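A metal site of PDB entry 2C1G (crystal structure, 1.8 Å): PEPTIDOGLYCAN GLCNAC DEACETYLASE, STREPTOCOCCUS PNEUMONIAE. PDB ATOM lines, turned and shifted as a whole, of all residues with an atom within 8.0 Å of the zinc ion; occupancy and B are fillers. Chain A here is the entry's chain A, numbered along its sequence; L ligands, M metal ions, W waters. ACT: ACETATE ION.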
ATOM      1  N   PHE A 242     -18.412  23.631  12.949  1.00  0.00           N
ATOM      2  CA  PHE A 242     -18.591  23.641  14.395  1.00  0.00           C
ATOM      3  C   PHE A 242     -18.905  22.258  14.875  1.00  0.00           C
ATOM      4  O   PHE A 242     -19.866  21.639  14.417  1.00  0.00           O
ATOM      5  CB  PHE A 242     -19.754  24.553  14.753  1.00  0.00           C
ATOM      6  CG  PHE A 242     -19.508  26.002  14.422  1.00  0.00           C
ATOM      7  CD1 PHE A 242     -18.753  26.806  15.279  1.00  0.00           C
ATOM      8  CD2 PHE A 242     -20.004  26.546  13.242  1.00  0.00           C
ATOM      9  CE1 PHE A 242     -18.500  28.152  14.948  1.00  0.00           C
ATOM     10  CE2 PHE A 242     -19.744  27.893  12.905  1.00  0.00           C
ATOM     11  CZ  PHE A 242     -18.985  28.688  13.762  1.00  0.00           C
ATOM     12  N   ASP A 243     -18.113  21.792  15.829  1.00  0.00           N
ATOM     13  CA  ASP A 243     -18.258  20.441  16.391  1.00  0.00           C
ATOM     14  C   ASP A 243     -18.845  20.398  17.803  1.00  0.00           C
ATOM     15  O   ASP A 243     -18.731  21.362  18.582  1.00  0.00           O
ATOM     16  CB  ASP A 243     -16.870  19.755  16.503  1.00  0.00           C
ATOM     17  CG  ASP A 243     -16.290  19.319  15.168  1.00  0.00           C
ATOM     18  OD1 ASP A 243     -16.890  19.596  14.113  1.00  0.00           O
ATOM     19  OD2 ASP A 243     -15.197  18.683  15.179  1.00  0.00           O
ATOM     20  N   ASP A 244     -19.378  19.206  18.106  1.00  0.00           N
ATOM     21  CA  ASP A 244     -19.878  18.787  19.413  1.00  0.00           C
ATOM     22  C   ASP A 244     -21.254  19.242  19.872  1.00  0.00           C
ATOM     23  O   ASP A 244     -21.662  18.913  20.990  1.00  0.00           O
ATOM     24  CB  ASP A 244     -18.871  19.138  20.531  1.00  0.00           C
ATOM     25  CG  ASP A 244     -17.475  18.487  20.366  1.00  0.00           C
ATOM     26  OD1 ASP A 244     -17.114  17.815  19.365  1.00  0.00           O
ATOM     27  OD2 ASP A 244     -16.670  18.653  21.306  1.00  0.00           O
ATOM     28  N   GLY A 245     -21.957  19.990  19.033  1.00  0.00           N
ATOM     29  CA  GLY A 245     -23.270  20.455  19.427  1.00  0.00           C
ATOM     30  C   GLY A 245     -24.377  19.479  19.089  1.00  0.00           C
ATOM     31  O   GLY A 245     -24.132  18.302  18.816  1.00  0.00           O
ATOM     32  N   PHE A 268     -21.082  19.745  12.775  1.00  0.00           N
ATOM     33  CA  PHE A 268     -20.914  18.302  12.956  1.00  0.00           C
ATOM     34  C   PHE A 268     -21.406  18.038  14.378  1.00  0.00           C
ATOM     35  O   PHE A 268     -20.713  18.293  15.364  1.00  0.00           O
ATOM     36  CB  PHE A 268     -19.449  17.908  12.748  1.00  0.00           C
ATOM     37  CG  PHE A 268     -19.023  17.966  11.299  1.00  0.00           C
ATOM     38  CD1 PHE A 268     -19.355  16.942  10.420  1.00  0.00           C
ATOM     39  CD2 PHE A 268     -18.345  19.086  10.791  1.00  0.00           C
ATOM     40  CE1 PHE A 268     -19.029  17.020   9.067  1.00  0.00           C
ATOM     41  CE2 PHE A 268     -18.015  19.177   9.431  1.00  0.00           C
ATOM     42  CZ  PHE A 268     -18.354  18.149   8.559  1.00  0.00           C
ATOM     43  N   LEU A 270     -23.214  15.803  17.623  1.00  0.00           N
ATOM     44  CA  LEU A 270     -23.151  14.510  18.306  1.00  0.00           C
ATOM     45  C   LEU A 270     -24.572  13.947  18.391  1.00  0.00           C
ATOM     46  O   LEU A 270     -25.510  14.645  18.801  1.00  0.00           O
ATOM     47  CB  LEU A 270     -22.571  14.666  19.721  1.00  0.00           C
ATOM     48  CG  LEU A 270     -21.044  14.879  19.782  1.00  0.00           C
ATOM     49  CD1 LEU A 270     -20.626  15.358  21.181  1.00  0.00           C
ATOM     50  CD2 LEU A 270     -20.336  13.578  19.413  1.00  0.00           C
ATOM     51  N   HIS A 294     -20.958  13.723  13.843  1.00  0.00           N
ATOM     52  CA  HIS A 294     -19.723  13.741  14.656  1.00  0.00           C
ATOM     53  C   HIS A 294     -19.665  12.532  15.615  1.00  0.00           C
ATOM     54  O   HIS A 294     -18.934  12.556  16.605  1.00  0.00           O
ATOM     55  CB  HIS A 294     -19.671  15.056  15.464  1.00  0.00           C
ATOM     56  CG  HIS A 294     -18.300  15.379  15.999  1.00  0.00           C
ATOM     57  ND1 HIS A 294     -17.140  15.103  15.313  1.00  0.00           N
ATOM     58  CD2 HIS A 294     -17.915  15.976  17.153  1.00  0.00           C
ATOM     59  CE1 HIS A 294     -16.096  15.506  16.022  1.00  0.00           C
ATOM     60  NE2 HIS A 294     -16.547  16.044  17.134  1.00  0.00           N
ATOM     61  N   SER A 295     -20.411  11.483  15.257  1.00  0.00           N
ATOM     62  CA  SER A 295     -20.551  10.248  16.025  1.00  0.00           C
ATOM     63  C   SER A 295     -21.657  10.450  17.044  1.00  0.00           C
ATOM     64  O   SER A 295     -22.212  11.542  17.179  1.00  0.00           O
ATOM     65  CB  SER A 295     -19.246   9.810  16.746  1.00  0.00           C
ATOM     66  OG  SER A 295     -19.036  10.494  17.968  1.00  0.00           O
ATOM     67  N   HIS A 298     -18.978  10.709  20.909  1.00  0.00           N
ATOM     68  CA  HIS A 298     -17.604  11.215  20.890  1.00  0.00           C
ATOM     69  C   HIS A 298     -16.474  10.290  21.366  1.00  0.00           C
ATOM     70  O   HIS A 298     -15.511  10.735  21.982  1.00  0.00           O
ATOM     71  CB  HIS A 298     -17.586  12.558  21.637  1.00  0.00           C
ATOM     72  CG  HIS A 298     -16.603  13.562  21.074  1.00  0.00           C
ATOM     73  ND1 HIS A 298     -15.250  13.529  21.345  1.00  0.00           N
ATOM     74  CD2 HIS A 298     -16.798  14.599  20.223  1.00  0.00           C
ATOM     75  CE1 HIS A 298     -14.650  14.509  20.694  1.00  0.00           C
ATOM     76  NE2 HIS A 298     -15.565  15.174  20.005  1.00  0.00           N
ATOM     77  N   ARG A 332     -17.462  13.714  10.527  1.00  0.00           N
ATOM     78  CA  ARG A 332     -16.184  14.122  11.082  1.00  0.00           C
ATOM     79  C   ARG A 332     -15.856  13.275  12.316  1.00  0.00           C
ATOM     80  O   ARG A 332     -16.560  13.334  13.318  1.00  0.00           O
ATOM     81  CB  ARG A 332     -16.184  15.574  11.521  1.00  0.00           C
ATOM     82  CG  ARG A 332     -14.857  15.897  12.194  1.00  0.00           C
ATOM     83  CD  ARG A 332     -14.681  17.372  12.389  1.00  0.00           C
ATOM     84  NE  ARG A 332     -14.395  18.035  11.117  1.00  0.00           N
ATOM     85  CZ  ARG A 332     -14.587  19.332  10.947  1.00  0.00           C
ATOM     86  NH1 ARG A 332     -15.059  20.039  11.958  1.00  0.00           N
ATOM     87  NH2 ARG A 332     -14.289  19.908   9.797  1.00  0.00           N
ATOM     88  N   PRO A 333     -14.787  12.478  12.253  1.00  0.00           N
ATOM     89  CA  PRO A 333     -14.397  11.618  13.380  1.00  0.00           C
ATOM     90  C   PRO A 333     -13.943  12.401  14.591  1.00  0.00           C
ATOM     91  O   PRO A 333     -13.189  13.371  14.474  1.00  0.00           O
ATOM     92  CB  PRO A 333     -13.215  10.811  12.817  1.00  0.00           C
ATOM     93  CG  PRO A 333     -13.526  10.740  11.350  1.00  0.00           C
ATOM     94  CD  PRO A 333     -14.004  12.153  11.053  1.00  0.00           C
ATOM     95  N   PRO A 334     -14.408  12.001  15.788  1.00  0.00           N
ATOM     96  CA  PRO A 334     -13.969  12.704  16.997  1.00  0.00           C
ATOM     97  C   PRO A 334     -12.433  12.598  16.995  1.00  0.00           C
ATOM     98  O   PRO A 334     -11.896  11.546  16.666  1.00  0.00           O
ATOM     99  CB  PRO A 334     -14.583  11.863  18.109  1.00  0.00           C
ATOM    100  CG  PRO A 334     -15.926  11.484  17.505  1.00  0.00           C
ATOM    101  CD  PRO A 334     -15.580  11.140  16.062  1.00  0.00           C
ATOM    102  N   TYR A 335     -11.751  13.698  17.347  1.00  0.00           N
ATOM    103  CA  TYR A 335     -10.286  13.784  17.430  1.00  0.00           C
ATOM    104  C   TYR A 335      -9.585  13.488  16.115  1.00  0.00           C
ATOM    105  O   TYR A 335      -8.371  13.340  16.074  1.00  0.00           O
ATOM    106  CB  TYR A 335      -9.748  12.804  18.494  1.00  0.00           C
ATOM    107  CG  TYR A 335     -10.544  12.788  19.786  1.00  0.00           C
ATOM    108  CD1 TYR A 335     -10.467  13.839  20.695  1.00  0.00           C
ATOM    109  CD2 TYR A 335     -11.421  11.737  20.061  1.00  0.00           C
ATOM    110  CE1 TYR A 335     -11.244  13.846  21.861  1.00  0.00           C
ATOM    111  CE2 TYR A 335     -12.202  11.741  21.205  1.00  0.00           C
ATOM    112  CZ  TYR A 335     -12.113  12.785  22.094  1.00  0.00           C
ATOM    113  OH  TYR A 335     -12.918  12.780  23.207  1.00  0.00           O
ATOM    114  N   GLY A 336     -10.351  13.396  15.043  1.00  0.00           N
ATOM    115  CA  GLY A 336      -9.767  13.080  13.759  1.00  0.00           C
ATOM    116  C   GLY A 336      -9.283  11.646  13.695  1.00  0.00           C
ATOM    117  O   GLY A 336      -8.511  11.307  12.806  1.00  0.00           O
ATOM    118  N   TRP A 353      -9.966  18.578   8.704  1.00  0.00           N
ATOM    119  CA  TRP A 353      -9.779  20.038   8.686  1.00  0.00           C
ATOM    120  C   TRP A 353      -8.292  20.333   8.466  1.00  0.00           C
ATOM    121  O   TRP A 353      -7.459  19.435   8.550  1.00  0.00           O
ATOM    122  CB  TRP A 353     -10.238  20.635  10.033  1.00  0.00           C
ATOM    123  CG  TRP A 353      -9.449  20.113  11.228  1.00  0.00           C
ATOM    124  CD1 TRP A 353      -8.259  20.614  11.717  1.00  0.00           C
ATOM    125  CD2 TRP A 353      -9.735  18.943  12.010  1.00  0.00           C
ATOM    126  NE1 TRP A 353      -7.792  19.820  12.738  1.00  0.00           N
ATOM    127  CE2 TRP A 353      -8.676  18.785  12.948  1.00  0.00           C
ATOM    128  CE3 TRP A 353     -10.780  18.012  12.013  1.00  0.00           C
ATOM    129  CZ2 TRP A 353      -8.641  17.736  13.862  1.00  0.00           C
ATOM    130  CZ3 TRP A 353     -10.742  16.953  12.927  1.00  0.00           C
ATOM    131  CH2 TRP A 353      -9.670  16.831  13.845  1.00  0.00           C
ATOM    132  N   TRP A 360     -11.031  25.041  21.598  1.00  0.00           N
ATOM    133  CA  TRP A 360     -11.251  24.032  22.643  1.00  0.00           C
ATOM    134  C   TRP A 360     -10.146  24.012  23.685  1.00  0.00           C
ATOM    135  O   TRP A 360     -10.343  23.503  24.788  1.00  0.00           O
ATOM    136  CB  TRP A 360     -11.343  22.625  22.038  1.00  0.00           C
ATOM    137  CG  TRP A 360     -10.123  22.205  21.208  1.00  0.00           C
ATOM    138  CD1 TRP A 360      -9.915  22.455  19.879  1.00  0.00           C
ATOM    139  CD2 TRP A 360      -8.971  21.490  21.665  1.00  0.00           C
ATOM    140  NE1 TRP A 360      -8.701  21.932  19.475  1.00  0.00           N
ATOM    141  CE2 TRP A 360      -8.094  21.340  20.559  1.00  0.00           C
ATOM    142  CE3 TRP A 360      -8.578  20.964  22.906  1.00  0.00           C
ATOM    143  CZ2 TRP A 360      -6.858  20.683  20.648  1.00  0.00           C
ATOM    144  CZ3 TRP A 360      -7.342  20.308  22.995  1.00  0.00           C
ATOM    145  CH2 TRP A 360      -6.501  20.176  21.871  1.00  0.00           C
ATOM    146  N   LEU A 383     -11.730  24.265  12.013  1.00  0.00           N
ATOM    147  CA  LEU A 383     -12.333  23.557  13.140  1.00  0.00           C
ATOM    148  C   LEU A 383     -12.614  24.478  14.326  1.00  0.00           C
ATOM    149  O   LEU A 383     -11.673  25.083  14.882  1.00  0.00           O
ATOM    150  CB  LEU A 383     -11.405  22.419  13.603  1.00  0.00           C
ATOM    151  CG  LEU A 383     -11.726  21.780  14.985  1.00  0.00           C
ATOM    152  CD1 LEU A 383     -13.095  21.104  14.962  1.00  0.00           C
ATOM    153  CD2 LEU A 383     -10.636  20.771  15.323  1.00  0.00           C
ATOM    154  N   MET A 384     -13.877  24.609  14.682  1.00  0.00           N
ATOM    155  CA  MET A 384     -14.337  25.359  15.865  1.00  0.00           C
ATOM    156  C   MET A 384     -15.384  24.498  16.614  1.00  0.00           C
ATOM    157  O   MET A 384     -15.791  23.450  16.125  1.00  0.00           O
ATOM    158  CB  MET A 384     -14.964  26.704  15.482  1.00  0.00           C
ATOM    159  CG  MET A 384     -13.987  27.614  14.719  1.00  0.00           C
ATOM    160  SD  MET A 384     -14.704  29.260  14.454  1.00  0.00           S
ATOM    161  CE  MET A 384     -15.426  29.056  12.812  1.00  0.00           C
ATOM    162  N   HIS A 385     -15.800  24.965  17.787  1.00  0.00           N
ATOM    163  CA  HIS A 385     -16.804  24.282  18.603  1.00  0.00           C
ATOM    164  C   HIS A 385     -17.867  25.296  19.022  1.00  0.00           C
ATOM    165  O   HIS A 385     -17.556  26.304  19.649  1.00  0.00           O
ATOM    166  CB  HIS A 385     -16.141  23.695  19.850  1.00  0.00           C
ATOM    167  CG  HIS A 385     -15.109  22.652  19.542  1.00  0.00           C
ATOM    168  ND1 HIS A 385     -13.852  22.961  19.078  1.00  0.00           N
ATOM    169  CD2 HIS A 385     -15.180  21.298  19.592  1.00  0.00           C
ATOM    170  CE1 HIS A 385     -13.198  21.837  18.824  1.00  0.00           C
ATOM    171  NE2 HIS A 385     -13.977  20.822  19.131  1.00  0.00           N
ATOM    172  N   ILE A 387     -20.001  25.068  21.316  1.00  0.00           N
ATOM    173  CA  ILE A 387     -20.551  24.725  22.611  1.00  0.00           C
ATOM    174  C   ILE A 387     -20.038  25.519  23.814  1.00  0.00           C
ATOM    175  O   ILE A 387     -20.546  25.323  24.914  1.00  0.00           O
ATOM    176  CB  ILE A 387     -20.391  23.219  22.884  1.00  0.00           C
ATOM    177  CG1 ILE A 387     -18.917  22.849  22.947  1.00  0.00           C
ATOM    178  CG2 ILE A 387     -21.089  22.414  21.763  1.00  0.00           C
ATOM    179  CD1 ILE A 387     -18.667  21.438  23.485  1.00  0.00           C
HETATM  180  C   ACT L   1     -13.328  17.027  17.187  1.00  0.00           C
HETATM  181  O   ACT L   1     -13.371  16.050  17.929  1.00  0.00           O
HETATM  182  OXT ACT L   1     -14.105  17.966  17.371  1.00  0.00           O
HETATM  183  CH3 ACT L   1     -12.321  17.072  16.037  1.00  0.00           C
HETATM  184 ZN    ZN M   1     -15.442  16.824  18.808  1.00  0.00          ZN
HETATM  185  O   HOH W   1     -14.410  17.921  20.283  1.00  0.00           O
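CB of Asp 243 touches the zinc ion (3.99 Å). Four residues have an atom within 4 Å of the zinc ion: Asp 243, Asp 244, His 294 and His 298. The nearest printed residue that does not touch the zinc ion is His 385 (4.3 Å).
The backbone NH of Asp 244 is in hydrogen-bond range of the backbone carbonyl oxygen of Phe 268, 3.2 Å away. ND1 of His 298 sits at hydrogen-bond distance from OH of Tyr 335, at 3.1 Å. The backbone NH of His 298 lies within hydrogen-bond range of the side-chain hydroxyl of Ser 295, 2.9 Å away. A ring nitrogen (ND1) of His 294 lies within hydrogen-bond range of the backbone carbonyl oxygen (O) of Arg 332 (2.7 Å). The side-chain carboxylate (OD1) of Asp 243 lies within salt-bridge range of the guanidinium group (NH1) of Arg 332, at 2.9 Å. O of Met 384 sits at hydrogen-bond distance from N of Asp 243 (2.9 Å).
Water W1 bridges the side-chain carboxylate of Asp 244 (2.6 Å) and a ring nitrogen (NE2) of His 385 (3.2 Å).
The zinc ion is bound by the side-chain carboxylate of Asp 244 (2.0 Å), a ring nitrogen (NE2) of His 298 (2.0 Å), water W1 (2.1 Å), a ring nitrogen (NE2) of His 294 (2.2 Å), an oxygen (OXT) of the ligand (2.3 Å) and an oxygen (O) of the ligand (2.4 Å).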
